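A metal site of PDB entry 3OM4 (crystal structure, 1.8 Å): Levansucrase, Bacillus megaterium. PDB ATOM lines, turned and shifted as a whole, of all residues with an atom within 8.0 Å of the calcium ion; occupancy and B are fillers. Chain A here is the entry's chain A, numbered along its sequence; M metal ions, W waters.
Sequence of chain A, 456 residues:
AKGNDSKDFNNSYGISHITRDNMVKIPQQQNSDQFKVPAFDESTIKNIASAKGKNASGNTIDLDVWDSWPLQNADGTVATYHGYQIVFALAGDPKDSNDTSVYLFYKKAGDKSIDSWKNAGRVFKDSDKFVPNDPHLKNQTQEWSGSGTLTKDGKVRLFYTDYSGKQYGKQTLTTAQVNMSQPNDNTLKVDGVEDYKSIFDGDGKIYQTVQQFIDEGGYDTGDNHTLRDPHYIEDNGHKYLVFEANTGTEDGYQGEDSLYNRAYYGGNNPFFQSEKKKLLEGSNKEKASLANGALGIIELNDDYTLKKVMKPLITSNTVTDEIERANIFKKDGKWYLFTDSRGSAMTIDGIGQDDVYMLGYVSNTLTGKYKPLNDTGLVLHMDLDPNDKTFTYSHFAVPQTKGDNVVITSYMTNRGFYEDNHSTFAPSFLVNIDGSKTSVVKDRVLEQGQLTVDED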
ATOM      1  N   GLN A 208     -20.268 -16.634  -9.421  1.00  0.00           N
ATOM      2  CA  GLN A 208     -20.546 -16.902  -8.009  1.00  0.00           C
ATOM      3  C   GLN A 208     -19.699 -16.014  -7.109  1.00  0.00           C
ATOM      4  O   GLN A 208     -18.529 -15.761  -7.391  1.00  0.00           O
ATOM      5  CB  GLN A 208     -20.282 -18.374  -7.693  1.00  0.00           C
ATOM      6  CG  GLN A 208     -20.743 -18.821  -6.312  1.00  0.00           C
ATOM      7  CD  GLN A 208     -20.172 -20.163  -5.910  1.00  0.00           C
ATOM      8  OE1 GLN A 208     -18.968 -20.399  -6.062  1.00  0.00           O
ATOM      9  NE2 GLN A 208     -21.017 -21.042  -5.393  1.00  0.00           N
ATOM     10  N   PHE A 213     -21.499 -18.841  -1.815  1.00  0.00           N
ATOM     11  CA  PHE A 213     -20.826 -20.066  -1.374  1.00  0.00           C
ATOM     12  C   PHE A 213     -21.109 -20.340   0.111  1.00  0.00           C
ATOM     13  O   PHE A 213     -21.501 -21.448   0.474  1.00  0.00           O
ATOM     14  CB  PHE A 213     -19.315 -19.954  -1.658  1.00  0.00           C
ATOM     15  CG  PHE A 213     -18.477 -20.990  -0.944  1.00  0.00           C
ATOM     16  CD1 PHE A 213     -18.335 -22.270  -1.452  1.00  0.00           C
ATOM     17  CD2 PHE A 213     -17.805 -20.656   0.230  1.00  0.00           C
ATOM     18  CE1 PHE A 213     -17.544 -23.219  -0.798  1.00  0.00           C
ATOM     19  CE2 PHE A 213     -17.021 -21.594   0.895  1.00  0.00           C
ATOM     20  CZ  PHE A 213     -16.892 -22.881   0.385  1.00  0.00           C
ATOM     21  N   THR A 221     -20.853 -28.988   2.149  1.00  0.00           N
ATOM     22  CA  THR A 221     -21.300 -29.730   0.964  1.00  0.00           C
ATOM     23  C   THR A 221     -20.157 -30.112   0.026  1.00  0.00           C
ATOM     24  O   THR A 221     -20.346 -30.898  -0.901  1.00  0.00           O
ATOM     25  CB  THR A 221     -22.328 -28.919   0.144  1.00  0.00           C
ATOM     26  OG1 THR A 221     -21.733 -27.681  -0.278  1.00  0.00           O
ATOM     27  CG2 THR A 221     -23.586 -28.640   0.951  1.00  0.00           C
ATOM     28  N   GLY A 222     -18.975 -29.543   0.265  1.00  0.00           N
ATOM     29  CA  GLY A 222     -17.825 -29.774  -0.593  1.00  0.00           C
ATOM     30  C   GLY A 222     -17.811 -28.905  -1.843  1.00  0.00           C
ATOM     31  O   GLY A 222     -17.131 -29.226  -2.813  1.00  0.00           O
ATOM     32  N   ASP A 223     -18.584 -27.825  -1.820  1.00  0.00           N
ATOM     33  CA  ASP A 223     -18.568 -26.845  -2.912  1.00  0.00           C
ATOM     34  C   ASP A 223     -17.190 -26.194  -2.990  1.00  0.00           C
ATOM     35  O   ASP A 223     -16.501 -26.068  -1.984  1.00  0.00           O
ATOM     36  CB  ASP A 223     -19.663 -25.780  -2.690  1.00  0.00           C
ATOM     37  CG  ASP A 223     -19.945 -24.957  -3.949  1.00  0.00           C
ATOM     38  OD1 ASP A 223     -19.812 -25.487  -5.071  1.00  0.00           O
ATOM     39  OD2 ASP A 223     -20.326 -23.779  -3.810  1.00  0.00           O
ATOM     40  N   ASN A 224     -16.795 -25.814  -4.198  1.00  0.00           N
ATOM     41  CA  ASN A 224     -15.504 -25.154  -4.383  1.00  0.00           C
ATOM     42  C   ASN A 224     -15.632 -23.808  -5.082  1.00  0.00           C
ATOM     43  O   ASN A 224     -15.836 -23.738  -6.298  1.00  0.00           O
ATOM     44  CB  ASN A 224     -14.537 -26.068  -5.139  1.00  0.00           C
ATOM     45  CG  ASN A 224     -13.120 -25.509  -5.201  1.00  0.00           C
ATOM     46  OD1 ASN A 224     -12.800 -24.507  -4.574  1.00  0.00           O
ATOM     47  ND2 ASN A 224     -12.264 -26.181  -5.960  1.00  0.00           N
ATOM     48  N   HIS A 225     -15.513 -22.749  -4.294  1.00  0.00           N
ATOM     49  CA  HIS A 225     -15.605 -21.400  -4.832  1.00  0.00           C
ATOM     50  C   HIS A 225     -14.260 -20.906  -5.352  1.00  0.00           C
ATOM     51  O   HIS A 225     -13.252 -20.979  -4.656  1.00  0.00           O
ATOM     52  CB  HIS A 225     -16.135 -20.422  -3.785  1.00  0.00           C
ATOM     53  CG  HIS A 225     -16.035 -18.991  -4.202  1.00  0.00           C
ATOM     54  ND1 HIS A 225     -16.855 -18.437  -5.163  1.00  0.00           N
ATOM     55  CD2 HIS A 225     -15.179 -18.005  -3.813  1.00  0.00           C
ATOM     56  CE1 HIS A 225     -16.520 -17.171  -5.344  1.00  0.00           C
ATOM     57  NE2 HIS A 225     -15.514 -16.884  -4.539  1.00  0.00           N
ATOM     58  N   THR A 226     -14.269 -20.410  -6.582  1.00  0.00           N
ATOM     59  CA  THR A 226     -13.068 -19.899  -7.244  1.00  0.00           C
ATOM     60  C   THR A 226     -13.347 -18.548  -7.901  1.00  0.00           C
ATOM     61  O   THR A 226     -14.451 -18.308  -8.395  1.00  0.00           O
ATOM     62  CB  THR A 226     -12.528 -20.877  -8.311  1.00  0.00           C
ATOM     63  OG1 THR A 226     -13.428 -20.910  -9.434  1.00  0.00           O
ATOM     64  CG2 THR A 226     -12.377 -22.296  -7.756  1.00  0.00           C
ATOM     65  N   ALA A 245     -13.545 -19.055 -12.648  1.00  0.00           N
ATOM     66  CA  ALA A 245     -14.647 -18.724 -11.760  1.00  0.00           C
ATOM     67  C   ALA A 245     -15.671 -19.859 -11.706  1.00  0.00           C
ATOM     68  O   ALA A 245     -15.378 -20.997 -12.089  1.00  0.00           O
ATOM     69  CB  ALA A 245     -15.306 -17.407 -12.183  1.00  0.00           C
ATOM     70  N   ASN A 246     -16.850 -19.520 -11.207  1.00  0.00           N
ATOM     71  CA  ASN A 246     -17.975 -20.437 -11.137  1.00  0.00           C
ATOM     72  C   ASN A 246     -19.219 -19.660 -11.549  1.00  0.00           C
ATOM     73  O   ASN A 246     -19.271 -18.451 -11.347  1.00  0.00           O
ATOM     74  CB  ASN A 246     -18.117 -20.993  -9.723  1.00  0.00           C
ATOM     75  CG  ASN A 246     -16.891 -21.772  -9.285  1.00  0.00           C
ATOM     76  OD1 ASN A 246     -15.973 -21.226  -8.680  1.00  0.00           O
ATOM     77  ND2 ASN A 246     -16.863 -23.060  -9.610  1.00  0.00           N
ATOM     78  N   THR A 247     -20.205 -20.339 -12.139  1.00  0.00           N
ATOM     79  CA  THR A 247     -21.406 -19.648 -12.609  1.00  0.00           C
ATOM     80  C   THR A 247     -22.197 -19.016 -11.471  1.00  0.00           C
ATOM     81  O   THR A 247     -22.180 -19.495 -10.322  1.00  0.00           O
ATOM     82  CB  THR A 247     -22.342 -20.568 -13.420  1.00  0.00           C
ATOM     83  OG1 THR A 247     -22.730 -21.694 -12.615  1.00  0.00           O
ATOM     84  CG2 THR A 247     -21.674 -21.056 -14.694  1.00  0.00           C
ATOM     85  N   TYR A 253     -26.722 -21.938 -12.909  1.00  0.00           N
ATOM     86  CA  TYR A 253     -26.253 -22.088 -11.538  1.00  0.00           C
ATOM     87  C   TYR A 253     -26.089 -23.555 -11.148  1.00  0.00           C
ATOM     88  O   TYR A 253     -26.736 -24.439 -11.715  1.00  0.00           O
ATOM     89  CB  TYR A 253     -27.217 -21.380 -10.572  1.00  0.00           C
ATOM     90  CG  TYR A 253     -26.630 -21.070  -9.200  1.00  0.00           C
ATOM     91  CD1 TYR A 253     -27.365 -21.344  -8.035  1.00  0.00           C
ATOM     92  CD2 TYR A 253     -25.359 -20.508  -9.066  1.00  0.00           C
ATOM     93  CE1 TYR A 253     -26.837 -21.046  -6.776  1.00  0.00           C
ATOM     94  CE2 TYR A 253     -24.831 -20.210  -7.806  1.00  0.00           C
ATOM     95  CZ  TYR A 253     -25.573 -20.482  -6.665  1.00  0.00           C
ATOM     96  OH  TYR A 253     -25.044 -20.181  -5.435  1.00  0.00           O
ATOM     97  N   GLN A 254     -25.227 -23.798 -10.170  1.00  0.00           N
ATOM     98  CA  GLN A 254     -25.072 -25.124  -9.579  1.00  0.00           C
ATOM     99  C   GLN A 254     -26.375 -25.568  -8.905  1.00  0.00           C
ATOM    100  O   GLN A 254     -27.246 -24.743  -8.620  1.00  0.00           O
ATOM    101  CB  GLN A 254     -23.932 -25.140  -8.566  1.00  0.00           C
ATOM    102  CG  GLN A 254     -24.160 -24.235  -7.364  1.00  0.00           C
ATOM    103  CD  GLN A 254     -22.929 -24.065  -6.516  1.00  0.00           C
ATOM    104  OE1 GLN A 254     -21.809 -24.059  -7.032  1.00  0.00           O
ATOM    105  NE2 GLN A 254     -23.127 -23.910  -5.215  1.00  0.00           N
ATOM    106  N   GLY A 255     -26.486 -26.864  -8.651  1.00  0.00           N
ATOM    107  CA  GLY A 255     -27.668 -27.441  -8.056  1.00  0.00           C
ATOM    108  C   GLY A 255     -28.146 -28.642  -8.836  1.00  0.00           C
ATOM    109  O   GLY A 255     -27.585 -28.977  -9.894  1.00  0.00           O
ATOM    110  N   GLU A 286     -24.098 -35.186  -5.649  1.00  0.00           N
ATOM    111  CA  GLU A 286     -23.804 -33.872  -5.093  1.00  0.00           C
ATOM    112  C   GLU A 286     -22.610 -33.221  -5.779  1.00  0.00           C
ATOM    113  O   GLU A 286     -22.667 -32.044  -6.121  1.00  0.00           O
ATOM    114  CB  GLU A 286     -23.568 -33.950  -3.577  1.00  0.00           C
ATOM    115  CG  GLU A 286     -23.406 -32.575  -2.934  1.00  0.00           C
ATOM    116  CD  GLU A 286     -23.024 -32.642  -1.477  1.00  0.00           C
ATOM    117  OE1 GLU A 286     -22.013 -33.292  -1.148  1.00  0.00           O
ATOM    118  OE2 GLU A 286     -23.742 -32.033  -0.649  1.00  0.00           O
ATOM    119  N   LYS A 287     -21.539 -33.985  -5.989  1.00  0.00           N
ATOM    120  CA  LYS A 287     -20.341 -33.484  -6.643  1.00  0.00           C
ATOM    121  C   LYS A 287     -20.644 -32.913  -8.033  1.00  0.00           C
ATOM    122  O   LYS A 287     -20.192 -31.816  -8.375  1.00  0.00           O
ATOM    123  CB  LYS A 287     -19.287 -34.592  -6.735  1.00  0.00           C
ATOM    124  CG  LYS A 287     -17.905 -34.125  -7.169  1.00  0.00           C
ATOM    125  CD  LYS A 287     -16.957 -35.316  -7.160  1.00  0.00           C
ATOM    126  CE  LYS A 287     -15.554 -34.919  -7.593  1.00  0.00           C
ATOM    127  NZ  LYS A 287     -14.676 -36.134  -7.630  1.00  0.00           N
ATOM    128  N   ALA A 288     -21.419 -33.656  -8.825  1.00  0.00           N
ATOM    129  CA  ALA A 288     -21.821 -33.185 -10.148  1.00  0.00           C
ATOM    130  C   ALA A 288     -22.728 -31.959 -10.059  1.00  0.00           C
ATOM    131  O   ALA A 288     -22.540 -30.986 -10.807  1.00  0.00           O
ATOM    132  CB  ALA A 288     -22.508 -34.314 -10.917  1.00  0.00           C
ATOM    133  N   SER A 289     -23.692 -31.987  -9.142  1.00  0.00           N
ATOM    134  CA  SER A 289     -24.616 -30.876  -8.936  1.00  0.00           C
ATOM    135  C   SER A 289     -23.873 -29.585  -8.613  1.00  0.00           C
ATOM    136  O   SER A 289     -24.183 -28.520  -9.164  1.00  0.00           O
ATOM    137  CB  SER A 289     -25.617 -31.187  -7.805  1.00  0.00           C
ATOM    138  OG  SER A 289     -26.482 -32.259  -8.153  1.00  0.00           O
ATOM    139  N   LEU A 290     -22.880 -29.686  -7.733  1.00  0.00           N
ATOM    140  CA  LEU A 290     -22.097 -28.527  -7.293  1.00  0.00           C
ATOM    141  C   LEU A 290     -21.066 -28.070  -8.317  1.00  0.00           C
ATOM    142  O   LEU A 290     -20.540 -26.956  -8.214  1.00  0.00           O
ATOM    143  CB  LEU A 290     -21.423 -28.802  -5.954  1.00  0.00           C
ATOM    144  CG  LEU A 290     -22.324 -28.944  -4.720  1.00  0.00           C
ATOM    145  CD1 LEU A 290     -21.474 -29.306  -3.520  1.00  0.00           C
ATOM    146  CD2 LEU A 290     -23.133 -27.683  -4.463  1.00  0.00           C
ATOM    147  N   ALA A 291     -20.763 -28.924  -9.292  1.00  0.00           N
ATOM    148  CA  ALA A 291     -19.787 -28.601 -10.335  1.00  0.00           C
ATOM    149  C   ALA A 291     -20.313 -27.549 -11.309  1.00  0.00           C
ATOM    150  O   ALA A 291     -21.174 -27.829 -12.143  1.00  0.00           O
ATOM    151  CB  ALA A 291     -19.360 -29.863 -11.087  1.00  0.00           C
ATOM    152  N   ASN A 292     -19.801 -26.322 -11.184  1.00  0.00           N
ATOM    153  CA  ASN A 292     -20.181 -25.232 -12.076  1.00  0.00           C
ATOM    154  C   ASN A 292     -18.997 -24.315 -12.434  1.00  0.00           C
ATOM    155  O   ASN A 292     -19.129 -23.087 -12.442  1.00  0.00           O
ATOM    156  CB  ASN A 292     -21.387 -24.443 -11.518  1.00  0.00           C
ATOM    157  CG  ASN A 292     -21.049 -23.633 -10.264  1.00  0.00           C
ATOM    158  OD1 ASN A 292     -20.176 -24.003  -9.482  1.00  0.00           O
ATOM    159  ND2 ASN A 292     -21.761 -22.525 -10.072  1.00  0.00           N
ATOM    160  N   GLY A 293     -17.851 -24.914 -12.722  1.00  0.00           N
ATOM    161  CA  GLY A 293     -16.677 -24.146 -13.146  1.00  0.00           C
ATOM    162  C   GLY A 293     -16.952 -23.312 -14.376  1.00  0.00           C
ATOM    163  O   GLY A 293     -17.781 -23.682 -15.218  1.00  0.00           O
ATOM    164  N   ASN A 317     -20.118 -27.118 -16.150  1.00  0.00           N
ATOM    165  CA  ASN A 317     -21.229 -27.596 -15.314  1.00  0.00           C
ATOM    166  C   ASN A 317     -21.341 -29.115 -15.339  1.00  0.00           C
ATOM    167  O   ASN A 317     -21.277 -29.723 -16.411  1.00  0.00           O
ATOM    168  CB  ASN A 317     -22.590 -27.020 -15.747  1.00  0.00           C
ATOM    169  CG  ASN A 317     -22.814 -25.587 -15.289  1.00  0.00           C
ATOM    170  OD1 ASN A 317     -23.443 -25.348 -14.251  1.00  0.00           O
ATOM    171  ND2 ASN A 317     -22.334 -24.640 -16.075  1.00  0.00           N
ATOM    172  N   THR A 320     -16.861 -30.485 -13.563  1.00  0.00           N
ATOM    173  CA  THR A 320     -15.934 -30.103 -12.513  1.00  0.00           C
ATOM    174  C   THR A 320     -16.197 -28.681 -12.023  1.00  0.00           C
ATOM    175  O   THR A 320     -16.709 -27.833 -12.757  1.00  0.00           O
ATOM    176  CB  THR A 320     -14.446 -30.217 -12.955  1.00  0.00           C
ATOM    177  OG1 THR A 320     -13.594 -29.859 -11.858  1.00  0.00           O
ATOM    178  CG2 THR A 320     -14.129 -29.324 -14.161  1.00  0.00           C
ATOM    179  N   ASP A 321     -15.845 -28.447 -10.761  1.00  0.00           N
ATOM    180  CA  ASP A 321     -15.937 -27.129 -10.161  1.00  0.00           C
ATOM    181  C   ASP A 321     -14.622 -26.365 -10.343  1.00  0.00           C
ATOM    182  O   ASP A 321     -14.543 -25.186 -10.021  1.00  0.00           O
ATOM    183  CB  ASP A 321     -16.253 -27.282  -8.673  1.00  0.00           C
ATOM    184  CG  ASP A 321     -17.351 -26.353  -8.225  1.00  0.00           C
ATOM    185  OD1 ASP A 321     -17.906 -25.613  -9.066  1.00  0.00           O
ATOM    186  OD2 ASP A 321     -17.673 -26.354  -7.019  1.00  0.00           O
ATOM    187  N   GLU A 322     -13.608 -27.056 -10.862  1.00  0.00           N
ATOM    188  CA  GLU A 322     -12.260 -26.494 -10.960  1.00  0.00           C
ATOM    189  C   GLU A 322     -11.641 -26.557 -12.358  1.00  0.00           C
ATOM    190  O   GLU A 322     -11.043 -27.562 -12.722  1.00  0.00           O
ATOM    191  CB  GLU A 322     -11.331 -27.239 -10.011  1.00  0.00           C
ATOM    192  CG  GLU A 322     -11.292 -26.669  -8.627  1.00  0.00           C
ATOM    193  CD  GLU A 322      -9.946 -26.825  -7.965  1.00  0.00           C
ATOM    194  OE1 GLU A 322      -9.613 -25.975  -7.114  1.00  0.00           O
ATOM    195  OE2 GLU A 322      -9.205 -27.792  -8.284  1.00  0.00           O
HETATM  196 CA    CA M   1     -19.701 -24.956  -7.387  1.00  0.00          CA
HETATM  197  O   HOH W   1     -18.467 -22.987  -6.897  1.00  0.00           O
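The side-chain amide oxygen of Asn 292 lies close to the side-chain amide nitrogen of Asn 246 (3.4 Å). The side-chain amide nitrogen (ND2) of Asn 292 sits at hydrogen-bond distance from the side-chain hydroxyl (OG1) of Thr 247. The side-chain carboxylate (OD2) of Asp 223 sits at hydrogen-bond distance from the side-chain amide nitrogen (NE2) of Gln 208 (3.2 Å). The side-chain amide nitrogen of Asn 246 sits at hydrogen-bond distance from the backbone carbonyl oxygen of Asp 321 (3.2 Å). N of Asn 224 lies close to OD2 of Asp 321 (3.0 Å).
Of the 26 residues printed, 5 come within 4 Å of the calcium ion. Along chain A the residues within 4 Å of the calcium ion span positions 223 to 321. The nearest printed residue that does not touch the calcium ion is Asn 246 (4.1 Å).
OE1 of Gln 254 binds the calcium ion (2.3 Å). The backbone carbonyl oxygen (O) of Leu 290 binds the calcium ion (2.3 Å). The calcium ion is bound by OD1 of Asn 292 (2.4 Å). Water W1 binds the calcium ion (2.4 Å). The calcium ion is bound by OD1 of Asp 223, at 2.4 Å. The side-chain carboxylate (OD2) of Asp 321 binds the calcium ion, 2.5 Å away. OD1 of Asp 321 is bound to the calcium ion (2.5 Å). The calcium ion has seven donor atoms within binding distance.
Water W1 lies within hydrogen-bond range of OE1 of Gln 208 (2.8 Å), O of Asn 224 (2.8 Å) and ND2 of Asn 246 (3.2 Å).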
